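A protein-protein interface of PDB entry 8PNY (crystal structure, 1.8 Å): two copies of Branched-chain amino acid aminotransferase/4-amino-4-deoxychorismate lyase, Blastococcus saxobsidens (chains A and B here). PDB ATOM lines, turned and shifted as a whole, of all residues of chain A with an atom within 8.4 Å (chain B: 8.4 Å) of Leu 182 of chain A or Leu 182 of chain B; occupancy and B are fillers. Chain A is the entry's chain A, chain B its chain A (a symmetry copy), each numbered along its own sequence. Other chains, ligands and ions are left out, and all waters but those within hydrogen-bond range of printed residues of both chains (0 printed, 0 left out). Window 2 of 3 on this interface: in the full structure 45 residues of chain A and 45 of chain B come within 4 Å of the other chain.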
ATOM      1  N   LEU A 135      26.984 -29.400  -0.459  1.00  0.00           N
ATOM      2  CA  LEU A 135      27.695 -28.409  -1.279  1.00  0.00           C
ATOM      3  C   LEU A 135      26.940 -28.273  -2.603  1.00  0.00           C
ATOM      4  O   LEU A 135      26.558 -29.306  -3.167  1.00  0.00           O
ATOM      5  CB  LEU A 135      29.145 -28.864  -1.482  1.00  0.00           C
ATOM      6  CG  LEU A 135      30.011 -28.966  -0.222  1.00  0.00           C
ATOM      7  CD1 LEU A 135      31.402 -29.501  -0.555  1.00  0.00           C
ATOM      8  CD2 LEU A 135      30.165 -27.620   0.492  1.00  0.00           C
ATOM      9  N   GLY A 136      26.692 -27.043  -3.045  1.00  0.00           N
ATOM     10  CA  GLY A 136      25.999 -26.842  -4.328  1.00  0.00           C
ATOM     11  C   GLY A 136      26.928 -27.137  -5.489  1.00  0.00           C
ATOM     12  O   GLY A 136      28.124 -26.847  -5.397  1.00  0.00           O
ATOM     13  N   LEU A 137      26.390 -27.730  -6.540  1.00  0.00           N
ATOM     14  CA  LEU A 137      27.072 -27.983  -7.825  1.00  0.00           C
ATOM     15  C   LEU A 137      26.819 -26.814  -8.771  1.00  0.00           C
ATOM     16  O   LEU A 137      27.507 -26.740  -9.783  1.00  0.00           O
ATOM     17  CB  LEU A 137      26.506 -29.287  -8.363  1.00  0.00           C
ATOM     18  CG  LEU A 137      27.518 -30.298  -8.861  1.00  0.00           C
ATOM     19  CD1 LEU A 137      28.694 -30.418  -7.903  1.00  0.00           C
ATOM     20  CD2 LEU A 137      26.836 -31.641  -9.084  1.00  0.00           C
ATOM     21  N   GLY A 138      25.866 -25.937  -8.452  1.00  0.00           N
ATOM     22  CA  GLY A 138      25.527 -24.767  -9.275  1.00  0.00           C
ATOM     23  C   GLY A 138      24.569 -25.071 -10.410  1.00  0.00           C
ATOM     24  O   GLY A 138      24.157 -24.150 -11.090  1.00  0.00           O
ATOM     25  N   VAL A 139      24.183 -26.315 -10.634  1.00  0.00           N
ATOM     26  CA  VAL A 139      23.375 -26.630 -11.843  1.00  0.00           C
ATOM     27  C   VAL A 139      21.927 -26.795 -11.419  1.00  0.00           C
ATOM     28  O   VAL A 139      21.655 -27.303 -10.338  1.00  0.00           O
ATOM     29  CB  VAL A 139      23.927 -27.860 -12.576  1.00  0.00           C
ATOM     30  CG1 VAL A 139      25.310 -27.558 -13.138  1.00  0.00           C
ATOM     31  CG2 VAL A 139      23.940 -29.096 -11.690  1.00  0.00           C
ATOM     32  N   PRO A 140      20.951 -26.352 -12.234  1.00  0.00           N
ATOM     33  CA  PRO A 140      19.565 -26.749 -12.028  1.00  0.00           C
ATOM     34  C   PRO A 140      19.420 -28.266 -12.078  1.00  0.00           C
ATOM     35  O   PRO A 140      20.154 -28.924 -12.805  1.00  0.00           O
ATOM     36  CB  PRO A 140      18.812 -26.099 -13.200  1.00  0.00           C
ATOM     37  CG  PRO A 140      19.674 -24.925 -13.528  1.00  0.00           C
ATOM     38  CD  PRO A 140      21.092 -25.442 -13.374  1.00  0.00           C
ATOM     39  N   ALA A 141      18.455 -28.770 -11.308  1.00  0.00           N
ATOM     40  CA  ALA A 141      18.133 -30.199 -11.155  1.00  0.00           C
ATOM     41  C   ALA A 141      17.811 -30.820 -12.523  1.00  0.00           C
ATOM     42  O   ALA A 141      18.260 -31.944 -12.742  1.00  0.00           O
ATOM     43  CB  ALA A 141      16.991 -30.339 -10.179  1.00  0.00           C
ATOM     44  N   ASP A 142      17.143 -30.075 -13.414  1.00  0.00           N
ATOM     45  CA  ASP A 142      16.674 -30.561 -14.739  1.00  0.00           C
ATOM     46  C   ASP A 142      17.713 -30.266 -15.827  1.00  0.00           C
ATOM     47  O   ASP A 142      17.416 -30.582 -16.977  1.00  0.00           O
ATOM     48  CB  ASP A 142      15.357 -29.899 -15.173  1.00  0.00           C
ATOM     49  CG  ASP A 142      14.180 -30.099 -14.226  1.00  0.00           C
ATOM     50  OD1 ASP A 142      14.178 -31.122 -13.494  1.00  0.00           O
ATOM     51  OD2 ASP A 142      13.259 -29.225 -14.232  1.00  0.00           O
ATOM     52  N   PHE A 143      18.874 -29.691 -15.518  1.00  0.00           N
ATOM     53  CA  PHE A 143      19.770 -29.154 -16.573  1.00  0.00           C
ATOM     54  C   PHE A 143      20.503 -30.286 -17.302  1.00  0.00           C
ATOM     55  O   PHE A 143      20.542 -30.265 -18.540  1.00  0.00           O
ATOM     56  CB  PHE A 143      20.768 -28.141 -16.029  1.00  0.00           C
ATOM     57  CG  PHE A 143      21.482 -27.426 -17.142  1.00  0.00           C
ATOM     58  CD1 PHE A 143      20.931 -26.285 -17.705  1.00  0.00           C
ATOM     59  CD2 PHE A 143      22.651 -27.941 -17.691  1.00  0.00           C
ATOM     60  CE1 PHE A 143      21.558 -25.632 -18.753  1.00  0.00           C
ATOM     61  CE2 PHE A 143      23.290 -27.281 -18.732  1.00  0.00           C
ATOM     62  CZ  PHE A 143      22.742 -26.127 -19.257  1.00  0.00           C
ATOM     63  N   PHE A 179      25.941 -33.437  -2.879  1.00  0.00           N
ATOM     64  CA  PHE A 179      25.757 -32.282  -3.793  1.00  0.00           C
ATOM     65  C   PHE A 179      24.281 -31.893  -3.850  1.00  0.00           C
ATOM     66  O   PHE A 179      23.379 -32.781  -3.817  1.00  0.00           O
ATOM     67  CB  PHE A 179      26.290 -32.558  -5.200  1.00  0.00           C
ATOM     68  CG  PHE A 179      27.792 -32.620  -5.301  1.00  0.00           C
ATOM     69  CD1 PHE A 179      28.566 -31.604  -4.781  1.00  0.00           C
ATOM     70  CD2 PHE A 179      28.430 -33.698  -5.903  1.00  0.00           C
ATOM     71  CE1 PHE A 179      29.947 -31.620  -4.909  1.00  0.00           C
ATOM     72  CE2 PHE A 179      29.814 -33.740  -5.996  1.00  0.00           C
ATOM     73  CZ  PHE A 179      30.569 -32.713  -5.485  1.00  0.00           C
ATOM     74  N   THR A 180      24.033 -30.591  -4.042  1.00  0.00           N
ATOM     75  CA  THR A 180      22.692 -30.010  -4.240  1.00  0.00           C
ATOM     76  C   THR A 180      22.639 -29.187  -5.528  1.00  0.00           C
ATOM     77  O   THR A 180      23.608 -28.522  -5.861  1.00  0.00           O
ATOM     78  CB  THR A 180      22.257 -29.151  -3.054  1.00  0.00           C
ATOM     79  OG1 THR A 180      23.259 -28.151  -2.893  1.00  0.00           O
ATOM     80  CG2 THR A 180      22.132 -29.977  -1.800  1.00  0.00           C
ATOM     81  N   SER A 181      21.515 -29.271  -6.207  1.00  0.00           N
ATOM     82  CA  SER A 181      21.181 -28.394  -7.352  1.00  0.00           C
ATOM     83  C   SER A 181      21.024 -26.939  -6.884  1.00  0.00           C
ATOM     84  O   SER A 181      21.047 -26.645  -5.666  1.00  0.00           O
ATOM     85  CB  SER A 181      19.915 -28.881  -7.977  1.00  0.00           C
ATOM     86  OG  SER A 181      18.818 -28.415  -7.200  1.00  0.00           O
ATOM     87  N   LEU A 182      20.808 -26.041  -7.843  1.00  0.00           N
ATOM     88  CA  LEU A 182      20.715 -24.589  -7.626  1.00  0.00           C
ATOM     89  C   LEU A 182      19.567 -24.271  -6.673  1.00  0.00           C
ATOM     90  O   LEU A 182      19.779 -23.429  -5.795  1.00  0.00           O
ATOM     91  CB  LEU A 182      20.484 -23.938  -8.992  1.00  0.00           C
ATOM     92  CG  LEU A 182      21.131 -22.576  -9.182  1.00  0.00           C
ATOM     93  CD1 LEU A 182      22.611 -22.646  -8.851  1.00  0.00           C
ATOM     94  CD2 LEU A 182      20.914 -22.083 -10.607  1.00  0.00           C
ATOM     95  N   GLU A 183      18.444 -24.966  -6.842  1.00  0.00           N
ATOM     96  CA  GLU A 183      17.157 -24.793  -6.120  1.00  0.00           C
ATOM     97  C   GLU A 183      17.209 -25.585  -4.804  1.00  0.00           C
ATOM     98  O   GLU A 183      16.244 -25.484  -4.045  1.00  0.00           O
ATOM     99  CB  GLU A 183      15.961 -25.289  -6.958  1.00  0.00           C
ATOM    100  CG  GLU A 183      16.065 -25.109  -8.485  1.00  0.00           C
ATOM    101  CD  GLU A 183      16.657 -26.256  -9.314  1.00  0.00           C
ATOM    102  OE1 GLU A 183      17.568 -26.911  -8.853  1.00  0.00           O
ATOM    103  OE2 GLU A 183      16.224 -26.449 -10.470  1.00  0.00           O
ATOM    104  N   GLY A 184      18.284 -26.329  -4.528  1.00  0.00           N
ATOM    105  CA  GLY A 184      18.504 -27.017  -3.238  1.00  0.00           C
ATOM    106  C   GLY A 184      18.064 -28.472  -3.244  1.00  0.00           C
ATOM    107  O   GLY A 184      18.037 -29.082  -2.153  1.00  0.00           O
ATOM    108  N   ARG A 185      17.785 -29.046  -4.422  1.00  0.00           N
ATOM    109  CA  ARG A 185      17.436 -30.478  -4.576  1.00  0.00           C
ATOM    110  C   ARG A 185      18.670 -31.337  -4.327  1.00  0.00           C
ATOM    111  O   ARG A 185      19.761 -30.968  -4.760  1.00  0.00           O
ATOM    112  CB  ARG A 185      16.896 -30.777  -5.974  1.00  0.00           C
ATOM    113  CG  ARG A 185      15.480 -30.265  -6.179  1.00  0.00           C
ATOM    114  CD  ARG A 185      14.507 -31.397  -6.418  1.00  0.00           C
ATOM    115  NE  ARG A 185      14.222 -31.625  -7.839  1.00  0.00           N
ATOM    116  CZ  ARG A 185      14.624 -32.678  -8.541  1.00  0.00           C
ATOM    117  NH1 ARG A 185      15.371 -33.615  -7.986  1.00  0.00           N
ATOM    118  NH2 ARG A 185      14.275 -32.791  -9.813  1.00  0.00           N
ATOM    119  N   LEU A 186      18.488 -32.445  -3.635  1.00  0.00           N
ATOM    120  CA  LEU A 186      19.556 -33.447  -3.465  1.00  0.00           C
ATOM    121  C   LEU A 186      19.914 -34.021  -4.836  1.00  0.00           C
ATOM    122  O   LEU A 186      19.010 -34.326  -5.645  1.00  0.00           O
ATOM    123  CB  LEU A 186      19.073 -34.546  -2.529  1.00  0.00           C
ATOM    124  CG  LEU A 186      18.704 -34.049  -1.143  1.00  0.00           C
ATOM    125  CD1 LEU A 186      18.143 -35.197  -0.327  1.00  0.00           C
ATOM    126  CD2 LEU A 186      19.912 -33.420  -0.457  1.00  0.00           C
ATOM    127  N   LEU A 187      21.207 -34.200  -5.063  1.00  0.00           N
ATOM    128  CA  LEU A 187      21.740 -34.961  -6.213  1.00  0.00           C
ATOM    129  C   LEU A 187      22.351 -36.260  -5.697  1.00  0.00           C
ATOM    130  O   LEU A 187      21.621 -37.275  -5.694  1.00  0.00           O
ATOM    131  CB  LEU A 187      22.719 -34.058  -6.956  1.00  0.00           C
ATOM    132  CG  LEU A 187      22.012 -32.858  -7.573  1.00  0.00           C
ATOM    133  CD1 LEU A 187      22.986 -31.853  -8.163  1.00  0.00           C
ATOM    134  CD2 LEU A 187      20.996 -33.333  -8.610  1.00  0.00           C
ATOM    135  N   LEU B 135      27.785 -23.860 -25.781  1.00  0.00           N
ATOM    136  CA  LEU B 135      27.185 -24.932 -24.975  1.00  0.00           C
ATOM    137  C   LEU B 135      27.065 -24.422 -23.538  1.00  0.00           C
ATOM    138  O   LEU B 135      28.027 -23.818 -23.050  1.00  0.00           O
ATOM    139  CB  LEU B 135      28.055 -26.191 -25.074  1.00  0.00           C
ATOM    140  CG  LEU B 135      28.184 -26.824 -26.464  1.00  0.00           C
ATOM    141  CD1 LEU B 135      29.136 -28.018 -26.435  1.00  0.00           C
ATOM    142  CD2 LEU B 135      26.837 -27.288 -27.022  1.00  0.00           C
ATOM    143  N   GLY B 136      25.905 -24.614 -22.913  1.00  0.00           N
ATOM    144  CA  GLY B 136      25.734 -24.177 -21.518  1.00  0.00           C
ATOM    145  C   GLY B 136      26.467 -25.108 -20.573  1.00  0.00           C
ATOM    146  O   GLY B 136      26.513 -26.315 -20.826  1.00  0.00           O
ATOM    147  N   LEU B 137      27.051 -24.549 -19.528  1.00  0.00           N
ATOM    148  CA  LEU B 137      27.696 -25.276 -18.416  1.00  0.00           C
ATOM    149  C   LEU B 137      26.677 -25.505 -17.304  1.00  0.00           C
ATOM    150  O   LEU B 137      26.968 -26.303 -16.419  1.00  0.00           O
ATOM    151  CB  LEU B 137      28.859 -24.413 -17.955  1.00  0.00           C
ATOM    152  CG  LEU B 137      30.181 -25.125 -17.760  1.00  0.00           C
ATOM    153  CD1 LEU B 137      30.465 -26.083 -18.907  1.00  0.00           C
ATOM    154  CD2 LEU B 137      31.297 -24.103 -17.593  1.00  0.00           C
ATOM    155  N   GLY B 138      25.527 -24.830 -17.350  1.00  0.00           N
ATOM    156  CA  GLY B 138      24.464 -24.965 -16.345  1.00  0.00           C
ATOM    157  C   GLY B 138      24.670 -24.106 -15.112  1.00  0.00           C
ATOM    158  O   GLY B 138      23.798 -24.079 -14.266  1.00  0.00           O
ATOM    159  N   VAL B 139      25.776 -23.393 -14.982  1.00  0.00           N
ATOM    160  CA  VAL B 139      26.048 -22.683 -13.703  1.00  0.00           C
ATOM    161  C   VAL B 139      25.727 -21.212 -13.897  1.00  0.00           C
ATOM    162  O   VAL B 139      25.952 -20.668 -14.972  1.00  0.00           O
ATOM    163  CB  VAL B 139      27.487 -22.923 -13.229  1.00  0.00           C
ATOM    164  CG1 VAL B 139      27.683 -24.391 -12.872  1.00  0.00           C
ATOM    165  CG2 VAL B 139      28.513 -22.453 -14.249  1.00  0.00           C
ATOM    166  N   PRO B 140      25.171 -20.523 -12.884  1.00  0.00           N
ATOM    167  CA  PRO B 140      25.123 -19.068 -12.904  1.00  0.00           C
ATOM    168  C   PRO B 140      26.524 -18.478 -13.016  1.00  0.00           C
ATOM    169  O   PRO B 140      27.474 -19.063 -12.508  1.00  0.00           O
ATOM    170  CB  PRO B 140      24.492 -18.695 -11.551  1.00  0.00           C
ATOM    171  CG  PRO B 140      23.679 -19.906 -11.230  1.00  0.00           C
ATOM    172  CD  PRO B 140      24.540 -21.071 -11.679  1.00  0.00           C
ATOM    173  N   ALA B 141      26.603 -17.319 -13.671  1.00  0.00           N
ATOM    174  CA  ALA B 141      27.838 -16.565 -13.943  1.00  0.00           C
ATOM    175  C   ALA B 141      28.562 -16.240 -12.627  1.00  0.00           C
ATOM    176  O   ALA B 141      29.787 -16.352 -12.626  1.00  0.00           O
ATOM    177  CB  ALA B 141      27.488 -15.322 -14.725  1.00  0.00           C
ATOM    178  N   ASP B 142      27.818 -15.944 -11.553  1.00  0.00           N
ATOM    179  CA  ASP B 142      28.367 -15.516 -10.238  1.00  0.00           C
ATOM    180  C   ASP B 142      28.560 -16.721  -9.310  1.00  0.00           C
ATOM    181  O   ASP B 142      28.967 -16.486  -8.174  1.00  0.00           O
ATOM    182  CB  ASP B 142      27.444 -14.524  -9.513  1.00  0.00           C
ATOM    183  CG  ASP B 142      27.145 -13.235 -10.269  1.00  0.00           C
ATOM    184  OD1 ASP B 142      27.990 -12.834 -11.110  1.00  0.00           O
ATOM    185  OD2 ASP B 142      26.062 -12.629 -10.002  1.00  0.00           O
ATOM    186  N   PHE B 143      28.291 -17.954  -9.735  1.00  0.00           N
ATOM    187  CA  PHE B 143      28.210 -19.093  -8.786  1.00  0.00           C
ATOM    188  C   PHE B 143      29.607 -19.533  -8.333  1.00  0.00           C
ATOM    189  O   PHE B 143      29.803 -19.729  -7.126  1.00  0.00           O
ATOM    190  CB  PHE B 143      27.442 -20.276  -9.360  1.00  0.00           C
ATOM    191  CG  PHE B 143      27.151 -21.303  -8.301  1.00  0.00           C
ATOM    192  CD1 PHE B 143      26.011 -21.196  -7.519  1.00  0.00           C
ATOM    193  CD2 PHE B 143      28.057 -22.320  -8.022  1.00  0.00           C
ATOM    194  CE1 PHE B 143      25.745 -22.115  -6.517  1.00  0.00           C
ATOM    195  CE2 PHE B 143      27.785 -23.251  -7.028  1.00  0.00           C
ATOM    196  CZ  PHE B 143      26.628 -23.146  -6.282  1.00  0.00           C
ATOM    197  N   PHE B 179      31.712 -21.952 -23.736  1.00  0.00           N
ATOM    198  CA  PHE B 179      30.720 -22.239 -22.669  1.00  0.00           C
ATOM    199  C   PHE B 179      29.948 -20.968 -22.320  1.00  0.00           C
ATOM    200  O   PHE B 179      30.529 -19.843 -22.312  1.00  0.00           O
ATOM    201  CB  PHE B 179      31.365 -22.832 -21.415  1.00  0.00           C
ATOM    202  CG  PHE B 179      31.861 -24.246 -21.574  1.00  0.00           C
ATOM    203  CD1 PHE B 179      31.031 -25.221 -22.087  1.00  0.00           C
ATOM    204  CD2 PHE B 179      33.160 -24.598 -21.223  1.00  0.00           C
ATOM    205  CE1 PHE B 179      31.455 -26.537 -22.193  1.00  0.00           C
ATOM    206  CE2 PHE B 179      33.603 -25.905 -21.368  1.00  0.00           C
ATOM    207  CZ  PHE B 179      32.758 -26.866 -21.867  1.00  0.00           C
ATOM    208  N   THR B 180      28.680 -21.151 -21.931  1.00  0.00           N
ATOM    209  CA  THR B 180      27.787 -20.083 -21.443  1.00  0.00           C
ATOM    210  C   THR B 180      27.209 -20.439 -20.073  1.00  0.00           C
ATOM    211  O   THR B 180      26.908 -21.597 -19.827  1.00  0.00           O
ATOM    212  CB  THR B 180      26.656 -19.785 -22.426  1.00  0.00           C
ATOM    213  OG1 THR B 180      25.964 -21.014 -22.627  1.00  0.00           O
ATOM    214  CG2 THR B 180      27.194 -19.263 -23.734  1.00  0.00           C
ATOM    215  N   SER B 181      27.086 -19.435 -19.232  1.00  0.00           N
ATOM    216  CA  SER B 181      26.353 -19.525 -17.949  1.00  0.00           C
ATOM    217  C   SER B 181      24.856 -19.757 -18.202  1.00  0.00           C
ATOM    218  O   SER B 181      24.382 -19.719 -19.361  1.00  0.00           O
ATOM    219  CB  SER B 181      26.562 -18.257 -17.186  1.00  0.00           C
ATOM    220  OG  SER B 181      25.685 -17.266 -17.707  1.00  0.00           O
ATOM    221  N   LEU B 182      24.107 -19.943 -17.118  1.00  0.00           N
ATOM    222  CA  LEU B 182      22.671 -20.267 -17.136  1.00  0.00           C
ATOM    223  C   LEU B 182      21.890 -19.160 -17.839  1.00  0.00           C
ATOM    224  O   LEU B 182      21.007 -19.507 -18.630  1.00  0.00           O
ATOM    225  CB  LEU B 182      22.218 -20.412 -15.681  1.00  0.00           C
ATOM    226  CG  LEU B 182      21.144 -21.459 -15.435  1.00  0.00           C
ATOM    227  CD1 LEU B 182      21.570 -22.796 -16.014  1.00  0.00           C
ATOM    228  CD2 LEU B 182      20.854 -21.577 -13.945  1.00  0.00           C
ATOM    229  N   GLU B 183      22.261 -17.910 -17.571  1.00  0.00           N
ATOM    230  CA  GLU B 183      21.616 -16.657 -18.043  1.00  0.00           C
ATOM    231  C   GLU B 183      22.160 -16.305 -19.436  1.00  0.00           C
ATOM    232  O   GLU B 183      21.669 -15.329 -20.007  1.00  0.00           O
ATOM    233  CB  GLU B 183      21.889 -15.479 -17.085  1.00  0.00           C
ATOM    234  CG  GLU B 183      22.002 -15.819 -15.587  1.00  0.00           C
ATOM    235  CD  GLU B 183      23.390 -16.134 -15.014  1.00  0.00           C
ATOM    236  OE1 GLU B 183      24.188 -16.741 -15.697  1.00  0.00           O
ATOM    237  OE2 GLU B 183      23.644 -15.808 -13.835  1.00  0.00           O
ATOM    238  N   GLY B 184      23.120 -17.063 -19.977  1.00  0.00           N
ATOM    239  CA  GLY B 184      23.617 -16.904 -21.360  1.00  0.00           C
ATOM    240  C   GLY B 184      24.870 -16.050 -21.459  1.00  0.00           C
ATOM    241  O   GLY B 184      25.258 -15.706 -22.597  1.00  0.00           O
ATOM    242  N   ARG B 185      25.530 -15.757 -20.331  1.00  0.00           N
ATOM    243  CA  ARG B 185      26.812 -15.013 -20.298  1.00  0.00           C
ATOM    244  C   ARG B 185      27.928 -15.891 -20.852  1.00  0.00           C
ATOM    245  O   ARG B 185      27.957 -17.087 -20.565  1.00  0.00           O
ATOM    246  CB  ARG B 185      27.176 -14.584 -18.877  1.00  0.00           C
ATOM    247  CG  ARG B 185      26.329 -13.425 -18.379  1.00  0.00           C
ATOM    248  CD  ARG B 185      27.166 -12.193 -18.121  1.00  0.00           C
ATOM    249  NE  ARG B 185      27.538 -12.029 -16.711  1.00  0.00           N
ATOM    250  CZ  ARG B 185      28.763 -12.177 -16.221  1.00  0.00           C
ATOM    251  NH1 ARG B 185      29.766 -12.533 -17.003  1.00  0.00           N
ATOM    252  NH2 ARG B 185      28.984 -11.970 -14.932  1.00  0.00           N
ATOM    253  N   LEU B 186      28.810 -15.299 -21.635  1.00  0.00           N
ATOM    254  CA  LEU B 186      30.028 -15.985 -22.102  1.00  0.00           C
ATOM    255  C   LEU B 186      30.899 -16.318 -20.891  1.00  0.00           C
ATOM    256  O   LEU B 186      31.069 -15.471 -19.987  1.00  0.00           O
ATOM    257  CB  LEU B 186      30.776 -15.081 -23.072  1.00  0.00           C
ATOM    258  CG  LEU B 186      29.973 -14.713 -24.307  1.00  0.00           C
ATOM    259  CD1 LEU B 186      30.764 -13.735 -25.152  1.00  0.00           C
ATOM    260  CD2 LEU B 186      29.603 -15.960 -25.101  1.00  0.00           C
ATOM    261  N   LEU B 187      31.469 -17.514 -20.906  1.00  0.00           N
ATOM    262  CA  LEU B 187      32.529 -17.929 -19.962  1.00  0.00           C
ATOM    263  C   LEU B 187      33.843 -18.051 -20.728  1.00  0.00           C
ATOM    264  O   LEU B 187      34.597 -17.054 -20.735  1.00  0.00           O
ATOM    265  CB  LEU B 187      32.074 -19.219 -19.287  1.00  0.00           C
ATOM    266  CG  LEU B 187      30.844 -18.989 -18.419  1.00  0.00           C
ATOM    267  CD1 LEU B 187      30.265 -20.285 -17.881  1.00  0.00           C
ATOM    268  CD2 LEU B 187      31.180 -18.012 -17.294  1.00  0.00           C
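Of the printed residues of chain B, Leu 182 of chain A touches Pro 140 (3.6 Å), Phe 143 (3.9 Å) and Leu 182 (3.4 Å).
No residue of chain B comes within 4 Å of Ser 181 of chain A.
Ser 181 of chain B touches none of the printed residues of chain A.
Printed residues of chain A within 4 Å of Phe 143 of chain B: Gly 136 (3.96 Å), Gly 138 (3.5 Å) and Leu 182 (3.9 Å).
Printed residues of chain B within 4 Å of Leu 137 of chain A: Val 139.
Of the printed residues of chain A, Gly 136 of chain B touches Phe 143.
The nearest residue of chain B that does not touch Leu 182 of chain A is Gly 138 of chain B (5.1 Å).
The nearest residue of chain A that does not touch Leu 182 of chain B is Gly 138 of chain A (5.1 Å).
The nearest printed residue of chain B that does not touch Pro 140 of chain A is Val 139 of chain B (5.4 Å).
Of the 18 printed residues of chain B, 7 touch a printed residue of chain A.
Hydrophobic or aromatic side chains of chain B within 4 Å of the printed part of chain A: Val 139, Pro 140, Phe 143 and Leu 182.
Among the printed residues, pairs that only touch across the chains: Gly 136 of chain A with Phe 143 of chain B (3.96 Å), Leu 137 of chain A with Val 139 of chain B (3.9 Å), Gly 138 of chain A with Val 139 of chain B (3.5 Å), Gly 138 of chain A with Pro 140 of chain B (3.2 Å), Gly 138 of chain A with Phe 143 of chain B (3.5 Å), Val 139 of chain A with Leu 137 of chain B (3.9 Å), Val 139 of chain A with Gly 138 of chain B (3.5 Å), Val 139 of chain A with Val 139 of chain B (3.97 Å), Pro 140 of chain A with Gly 138 of chain B (3.2 Å), Pro 140 of chain A with Leu 182 of chain B (3.6 Å), Phe 143 of chain A with Gly 136 of chain B (3.96 Å), Phe 143 of chain A with Gly 138 of chain B (3.5 Å), Phe 143 of chain A with Leu 182 of chain B (3.9 Å), Leu 182 of chain A with Pro 140 of chain B (3.6 Å), Leu 182 of chain A with Phe 143 of chain B (3.9 Å) and Leu 182 of chain A with Leu 182 of chain B (3.4 Å).
Gly 138 of chain A touches its own counterpart, Gly 138 of chain B.
Gly 138 of chain A touches Pro 140 of chain B, and with the chains exchanged Pro 140 of chain A touches Gly 138 of chain B.
Val 139 of chain B touches its own counterpart, Val 139 of chain A.
Leu 182 of chain A touches its own counterpart, Leu 182 of chain B.
Positions printed for both chains: 135, 136, 137, 138, 139, 140, 141, 142, 143, 179, 180, 181, 182, 183, 184, 185, 186 and 187.
Of the 17 pairs that touch across the chains among the printed residues, 17 have their exchanged pair printed and touching as well.
N of Leu 137 of chain A is in hydrogen-bond range of O of Thr 180 of chain A (3.0 Å).
The backbone carbonyl oxygen of Val 139 of chain A sits at hydrogen-bond distance from the backbone NH of Leu 182 of chain A, at 2.9 Å.
The backbone NH (N) of Leu 137 of chain B sits at hydrogen-bond distance from the backbone carbonyl oxygen (O) of Thr 180 of chain B (3.0 Å).
N of Leu 182 of chain B sits at hydrogen-bond distance from O of Val 139 of chain B, at 2.9 Å.
The backbone carbonyl oxygen of Gly 138 of chain A lies close to the backbone carbonyl oxygen of Gly 138 of chain B (3.2 Å).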
